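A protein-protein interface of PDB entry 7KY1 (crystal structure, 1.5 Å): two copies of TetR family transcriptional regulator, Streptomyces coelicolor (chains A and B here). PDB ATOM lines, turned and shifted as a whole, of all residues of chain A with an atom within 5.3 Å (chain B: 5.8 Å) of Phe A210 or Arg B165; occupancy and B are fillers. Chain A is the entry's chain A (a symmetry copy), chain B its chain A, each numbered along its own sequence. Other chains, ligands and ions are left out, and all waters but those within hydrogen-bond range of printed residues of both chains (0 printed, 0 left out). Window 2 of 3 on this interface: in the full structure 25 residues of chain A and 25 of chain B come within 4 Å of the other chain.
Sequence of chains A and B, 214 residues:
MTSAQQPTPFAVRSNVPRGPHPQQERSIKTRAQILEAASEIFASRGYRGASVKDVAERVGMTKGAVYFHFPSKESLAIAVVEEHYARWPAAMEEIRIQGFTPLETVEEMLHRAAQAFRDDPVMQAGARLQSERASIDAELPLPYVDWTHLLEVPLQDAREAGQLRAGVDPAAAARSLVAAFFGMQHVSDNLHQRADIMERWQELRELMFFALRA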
ATOM      1  N   ARG A 205      19.589 -21.068  12.331  1.00  0.00           N
ATOM      2  CA  ARG A 205      19.566 -21.909  13.528  1.00  0.00           C
ATOM      3  C   ARG A 205      20.368 -21.291  14.668  1.00  0.00           C
ATOM      4  O   ARG A 205      19.912 -21.227  15.815  1.00  0.00           O
ATOM      5  CB  ARG A 205      20.137 -23.295  13.177  1.00  0.00           C
ATOM      6  CG  ARG A 205      20.277 -24.264  14.362  1.00  0.00           C
ATOM      7  CD  ARG A 205      21.366 -25.336  14.133  1.00  0.00           C
ATOM      8  NE  ARG A 205      22.714 -24.759  14.186  1.00  0.00           N
ATOM      9  CZ  ARG A 205      23.290 -24.279  15.288  1.00  0.00           C
ATOM     10  NH1 ARG A 205      22.644 -24.285  16.450  1.00  0.00           N
ATOM     11  NH2 ARG A 205      24.515 -23.771  15.231  1.00  0.00           N
ATOM     12  N   GLU A 206      21.593 -20.868  14.383  1.00  0.00           N
ATOM     13  CA  GLU A 206      22.401 -20.267  15.437  1.00  0.00           C
ATOM     14  C   GLU A 206      21.699 -19.087  16.095  1.00  0.00           C
ATOM     15  O   GLU A 206      21.765 -18.929  17.317  1.00  0.00           O
ATOM     16  CB  GLU A 206      23.751 -19.815  14.876  1.00  0.00           C
ATOM     17  CG  GLU A 206      24.787 -19.443  15.958  1.00  0.00           C
ATOM     18  CD  GLU A 206      24.636 -18.041  16.591  1.00  0.00           C
ATOM     19  OE1 GLU A 206      24.003 -17.132  16.003  1.00  0.00           O
ATOM     20  OE2 GLU A 206      25.193 -17.846  17.696  1.00  0.00           O
ATOM     21  N   LEU A 207      21.088 -18.208  15.303  1.00  0.00           N
ATOM     22  CA  LEU A 207      20.370 -17.070  15.864  1.00  0.00           C
ATOM     23  C   LEU A 207      19.167 -17.514  16.678  1.00  0.00           C
ATOM     24  O   LEU A 207      18.993 -17.106  17.834  1.00  0.00           O
ATOM     25  CB  LEU A 207      19.909 -16.141  14.747  1.00  0.00           C
ATOM     26  CG  LEU A 207      20.989 -15.376  14.012  1.00  0.00           C
ATOM     27  CD1 LEU A 207      20.253 -14.521  12.982  1.00  0.00           C
ATOM     28  CD2 LEU A 207      21.795 -14.507  14.991  1.00  0.00           C
ATOM     29  N   MET A 208      18.305 -18.322  16.071  1.00  0.00           N
ATOM     30  CA  MET A 208      17.065 -18.656  16.746  1.00  0.00           C
ATOM     31  C   MET A 208      17.327 -19.461  18.016  1.00  0.00           C
ATOM     32  O   MET A 208      16.719 -19.182  19.053  1.00  0.00           O
ATOM     33  CB  MET A 208      16.132 -19.379  15.776  1.00  0.00           C
ATOM     34  CG  MET A 208      15.839 -18.527  14.529  1.00  0.00           C
ATOM     35  SD  MET A 208      14.339 -18.986  13.646  1.00  0.00           S
ATOM     36  CE  MET A 208      13.043 -18.462  14.790  1.00  0.00           C
ATOM     37  N   PHE A 209      18.243 -20.413  17.982  1.00  0.00           N
ATOM     38  CA  PHE A 209      18.423 -21.170  19.214  1.00  0.00           C
ATOM     39  C   PHE A 209      19.233 -20.413  20.253  1.00  0.00           C
ATOM     40  O   PHE A 209      19.066 -20.659  21.450  1.00  0.00           O
ATOM     41  CB  PHE A 209      18.991 -22.542  18.877  1.00  0.00           C
ATOM     42  CG  PHE A 209      17.932 -23.465  18.360  1.00  0.00           C
ATOM     43  CD1 PHE A 209      17.570 -23.439  17.034  1.00  0.00           C
ATOM     44  CD2 PHE A 209      17.204 -24.266  19.236  1.00  0.00           C
ATOM     45  CE1 PHE A 209      16.532 -24.253  16.551  1.00  0.00           C
ATOM     46  CE2 PHE A 209      16.173 -25.081  18.766  1.00  0.00           C
ATOM     47  CZ  PHE A 209      15.839 -25.077  17.430  1.00  0.00           C
ATOM     48  N   PHE A 210      20.069 -19.453  19.853  1.00  0.00           N
ATOM     49  CA  PHE A 210      20.649 -18.564  20.854  1.00  0.00           C
ATOM     50  C   PHE A 210      19.551 -17.846  21.624  1.00  0.00           C
ATOM     51  O   PHE A 210      19.653 -17.637  22.845  1.00  0.00           O
ATOM     52  CB  PHE A 210      21.594 -17.545  20.201  1.00  0.00           C
ATOM     53  CG  PHE A 210      22.197 -16.577  21.184  1.00  0.00           C
ATOM     54  CD1 PHE A 210      21.542 -15.410  21.541  1.00  0.00           C
ATOM     55  CD2 PHE A 210      23.420 -16.862  21.771  1.00  0.00           C
ATOM     56  CE1 PHE A 210      22.101 -14.523  22.478  1.00  0.00           C
ATOM     57  CE2 PHE A 210      23.987 -15.971  22.699  1.00  0.00           C
ATOM     58  CZ  PHE A 210      23.325 -14.812  23.043  1.00  0.00           C
ATOM     59  N   ALA A 211      18.474 -17.494  20.932  1.00  0.00           N
ATOM     60  CA  ALA A 211      17.401 -16.754  21.566  1.00  0.00           C
ATOM     61  C   ALA A 211      16.443 -17.643  22.352  1.00  0.00           C
ATOM     62  O   ALA A 211      15.723 -17.135  23.217  1.00  0.00           O
ATOM     63  CB  ALA A 211      16.626 -15.969  20.504  1.00  0.00           C
ATOM     64  N   LEU A 212      16.425 -18.951  22.090  1.00  0.00           N
ATOM     65  CA  LEU A 212      15.543 -19.859  22.834  1.00  0.00           C
ATOM     66  C   LEU A 212      16.186 -20.454  24.081  1.00  0.00           C
ATOM     67  O   LEU A 212      15.465 -20.738  25.050  1.00  0.00           O
ATOM     68  CB  LEU A 212      15.081 -21.000  21.929  1.00  0.00           C
ATOM     69  CG  LEU A 212      14.179 -20.561  20.774  1.00  0.00           C
ATOM     70  CD1 LEU A 212      14.000 -21.707  19.791  1.00  0.00           C
ATOM     71  CD2 LEU A 212      12.846 -20.034  21.299  1.00  0.00           C
ATOM     72  N   ARG A 213      17.500 -20.687  24.086  1.00  0.00           N
ATOM     73  CA  ARG A 213      18.117 -21.414  25.191  1.00  0.00           C
ATOM     74  C   ARG A 213      18.124 -20.566  26.450  1.00  0.00           C
ATOM     75  O   ARG A 213      18.399 -19.364  26.407  1.00  0.00           O
ATOM     76  CB  ARG A 213      19.558 -21.800  24.866  1.00  0.00           C
ATOM     77  CG  ARG A 213      19.713 -22.778  23.767  1.00  0.00           C
ATOM     78  CD  ARG A 213      21.146 -23.288  23.714  1.00  0.00           C
ATOM     79  NE  ARG A 213      21.370 -24.009  22.467  1.00  0.00           N
ATOM     80  CZ  ARG A 213      21.910 -23.470  21.379  1.00  0.00           C
ATOM     81  NH1 ARG A 213      22.061 -24.218  20.288  1.00  0.00           N
ATOM     82  NH2 ARG A 213      22.316 -22.197  21.385  1.00  0.00           N
ATOM     83  N   GLN B 163      26.977  -2.653  18.320  1.00  0.00           N
ATOM     84  CA  GLN B 163      25.585  -2.921  18.651  1.00  0.00           C
ATOM     85  C   GLN B 163      25.181  -4.359  18.385  1.00  0.00           C
ATOM     86  O   GLN B 163      24.123  -4.784  18.853  1.00  0.00           O
ATOM     87  CB  GLN B 163      24.679  -1.974  17.868  1.00  0.00           C
ATOM     88  CG  GLN B 163      24.846  -0.550  18.391  1.00  0.00           C
ATOM     89  CD  GLN B 163      24.214   0.523  17.518  1.00  0.00           C
ATOM     90  OE1 GLN B 163      23.464   0.241  16.564  1.00  0.00           O
ATOM     91  NE2 GLN B 163      24.514   1.773  17.853  1.00  0.00           N
ATOM     92  N   LEU B 164      26.008  -5.118  17.672  1.00  0.00           N
ATOM     93  CA  LEU B 164      25.720  -6.506  17.342  1.00  0.00           C
ATOM     94  C   LEU B 164      26.505  -7.457  18.229  1.00  0.00           C
ATOM     95  O   LEU B 164      27.680  -7.223  18.537  1.00  0.00           O
ATOM     96  CB  LEU B 164      26.069  -6.814  15.887  1.00  0.00           C
ATOM     97  CG  LEU B 164      25.168  -6.478  14.727  1.00  0.00           C
ATOM     98  CD1 LEU B 164      25.709  -7.235  13.510  1.00  0.00           C
ATOM     99  CD2 LEU B 164      23.722  -6.860  15.010  1.00  0.00           C
ATOM    100  N   ARG B 165      25.862  -8.555  18.600  1.00  0.00           N
ATOM    101  CA  ARG B 165      26.531  -9.576  19.384  1.00  0.00           C
ATOM    102  C   ARG B 165      27.789 -10.050  18.660  1.00  0.00           C
ATOM    103  O   ARG B 165      27.810 -10.172  17.431  1.00  0.00           O
ATOM    104  CB  ARG B 165      25.579 -10.745  19.640  1.00  0.00           C
ATOM    105  CG  ARG B 165      26.244 -11.960  20.253  1.00  0.00           C
ATOM    106  CD  ARG B 165      25.230 -12.938  20.779  1.00  0.00           C
ATOM    107  NE  ARG B 165      24.281 -13.354  19.757  1.00  0.00           N
ATOM    108  CZ  ARG B 165      24.408 -14.465  19.036  1.00  0.00           C
ATOM    109  NH1 ARG B 165      25.453 -15.262  19.234  1.00  0.00           N
ATOM    110  NH2 ARG B 165      23.494 -14.781  18.130  1.00  0.00           N
ATOM    111  N   ALA B 166      28.847 -10.293  19.438  1.00  0.00           N
ATOM    112  CA  ALA B 166      30.115 -10.752  18.889  1.00  0.00           C
ATOM    113  C   ALA B 166      29.925 -12.071  18.155  1.00  0.00           C
ATOM    114  O   ALA B 166      29.268 -12.989  18.651  1.00  0.00           O
ATOM    115  CB  ALA B 166      31.146 -10.911  20.007  1.00  0.00           C
ATOM    116  N   GLY B 167      30.499 -12.164  16.974  1.00  0.00           N
ATOM    117  CA  GLY B 167      30.373 -13.353  16.176  1.00  0.00           C
ATOM    118  C   GLY B 167      29.243 -13.318  15.178  1.00  0.00           C
ATOM    119  O   GLY B 167      29.229 -14.153  14.271  1.00  0.00           O
ATOM    120  N   VAL B 168      28.300 -12.386  15.302  1.00  0.00           N
ATOM    121  CA  VAL B 168      27.214 -12.306  14.328  1.00  0.00           C
ATOM    122  C   VAL B 168      27.711 -11.553  13.105  1.00  0.00           C
ATOM    123  O   VAL B 168      28.127 -10.395  13.211  1.00  0.00           O
ATOM    124  CB  VAL B 168      25.970 -11.620  14.909  1.00  0.00           C
ATOM    125  CG1 VAL B 168      24.953 -11.391  13.778  1.00  0.00           C
ATOM    126  CG2 VAL B 168      25.338 -12.464  16.014  1.00  0.00           C
ATOM    127  N   PHE B 210      16.621 -10.360  20.032  1.00  0.00           N
ATOM    128  CA  PHE B 210      17.347 -10.798  21.221  1.00  0.00           C
ATOM    129  C   PHE B 210      18.670 -11.438  20.826  1.00  0.00           C
ATOM    130  O   PHE B 210      19.698 -11.256  21.500  1.00  0.00           O
ATOM    131  CB  PHE B 210      16.505 -11.780  22.047  1.00  0.00           C
ATOM    132  CG  PHE B 210      17.220 -12.293  23.270  1.00  0.00           C
ATOM    133  CD1 PHE B 210      18.051 -13.399  23.209  1.00  0.00           C
ATOM    134  CD2 PHE B 210      17.069 -11.636  24.482  1.00  0.00           C
ATOM    135  CE1 PHE B 210      18.733 -13.856  24.351  1.00  0.00           C
ATOM    136  CE2 PHE B 210      17.740 -12.099  25.627  1.00  0.00           C
ATOM    137  CZ  PHE B 210      18.563 -13.202  25.553  1.00  0.00           C
ATOM    138  N   ALA B 211      18.670 -12.163  19.714  1.00  0.00           N
ATOM    139  CA  ALA B 211      19.867 -12.860  19.289  1.00  0.00           C
ATOM    140  C   ALA B 211      20.851 -11.962  18.547  1.00  0.00           C
ATOM    141  O   ALA B 211      22.032 -12.309  18.454  1.00  0.00           O
ATOM    142  CB  ALA B 211      19.480 -14.047  18.403  1.00  0.00           C
ATOM    143  N   LEU B 212      20.406 -10.813  18.033  1.00  0.00           N
ATOM    144  CA  LEU B 212      21.314  -9.897  17.332  1.00  0.00           C
ATOM    145  C   LEU B 212      21.957  -8.857  18.240  1.00  0.00           C
ATOM    146  O   LEU B 212      23.088  -8.431  17.957  1.00  0.00           O
ATOM    147  CB  LEU B 212      20.567  -9.175  16.212  1.00  0.00           C
ATOM    148  CG  LEU B 212      20.102 -10.087  15.075  1.00  0.00           C
ATOM    149  CD1 LEU B 212      19.148  -9.332  14.161  1.00  0.00           C
ATOM    150  CD2 LEU B 212      21.296 -10.662  14.319  1.00  0.00           C
ATOM    151  N   ARG B 213      21.276  -8.405  19.295  1.00  0.00           N
ATOM    152  CA  ARG B 213      21.788  -7.287  20.082  1.00  0.00           C
ATOM    153  C   ARG B 213      23.009  -7.710  20.879  1.00  0.00           C
ATOM    154  O   ARG B 213      23.049  -8.803  21.450  1.00  0.00           O
ATOM    155  CB  ARG B 213      20.736  -6.766  21.058  1.00  0.00           C
ATOM    156  CG  ARG B 213      19.549  -6.146  20.429  1.00  0.00           C
ATOM    157  CD  ARG B 213      18.711  -5.430  21.478  1.00  0.00           C
ATOM    158  NE  ARG B 213      17.410  -5.081  20.921  1.00  0.00           N
ATOM    159  CZ  ARG B 213      16.311  -5.813  21.072  1.00  0.00           C
ATOM    160  NH1 ARG B 213      15.174  -5.407  20.511  1.00  0.00           N
ATOM    161  NH2 ARG B 213      16.342  -6.936  21.798  1.00  0.00           N
ATOM    162  N   ALA B 214      23.987  -6.812  20.971  1.00  0.00           N
ATOM    163  CA  ALA B 214      25.125  -7.039  21.844  1.00  0.00           C
ATOM    164  C   ALA B 214      24.654  -7.160  23.292  1.00  0.00           C
ATOM    165  O   ALA B 214      23.648  -6.558  23.695  1.00  0.00           O
ATOM    166  CB  ALA B 214      26.123  -5.911  21.709  1.00  0.00           C
ATOM    167  OXT ALA B 214      25.288  -7.855  24.084  1.00  0.00           O
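The side-chain carboxylate (OE2) of Glu A206 lies within salt-bridge range of the guanidinium group (NH1) of Arg B165, at 3.0 Å.
The backbone NH of Arg B165 lies within hydrogen-bond range of the backbone carbonyl oxygen of Leu B212, 2.9 Å away.
NE of Arg B165 sits at hydrogen-bond distance from O of Ala B211, at 2.8 Å.
CD2 of Leu A207 touches NH2 of Arg B165 (3.6 Å).
CB of Ala B211 touches O of Leu A207 (3.1 Å).
CD2 of Leu A207 touches CD2 of Leu B212, at 3.9 Å.
Phe A210 touches Arg B165.
CE1 of Phe A210 touches CE1 of Phe B210 (3.9 Å).
CD1 of Phe A210 touches CA of Ala B211 (3.8 Å).
Ala A211 touches Phe B210 (CA to CD1, 3.8 Å).
Of the printed residues of chain B, Leu A207 touches Arg B165 (3.6 Å), Ala B211 (3.1 Å) and Leu B212 (3.9 Å).
Of chain B, only Arg B165 (3.5 Å), Phe B210 (3.9 Å) and Ala B211 (3.8 Å) come within 4 Å of Phe A210.
Of chain A, only Glu A206 (3.0 Å), Leu A207 (3.6 Å) and Phe A210 (3.5 Å) come within 4 Å of Arg B165.
Of the printed residues of chain A, Phe B210 touches Phe A210 and Ala A211.
Printed residues of chain A within 4 Å of Leu B212: Leu A207 (3.9 Å).
The nearest printed residue of chain B that does not touch Phe A210 is Arg B213 (5.9 Å).
The nearest printed residue of chain A that does not touch Ala B211 is Ala A211 (4.03 Å).
Printed residues of chain A that touch a printed residue of chain B: Glu A206, Leu A207, Phe A210 and Ala A211.
Hydrophobic or aromatic side chains of chain A within 4 Å of the printed part of chain B: Leu A207, Phe A210 and Ala A211.
Of the 11 printed residues of chain B, 4 touch a printed residue of chain A.
Hydrophobic or aromatic side chains of chain B that line the printed part of chain A: Phe B210, Ala B211 and Leu B212.
Among the printed residues, 8 pairs touch across the chains.
Phe A210 touches its own counterpart, Phe B210.
Phe A210 touches Ala B211, and with the chains exchanged Ala A211 touches Phe B210.
Of the 8 pairs that touch across the chains among the printed residues, 3 have their exchanged pair printed and touching as well.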
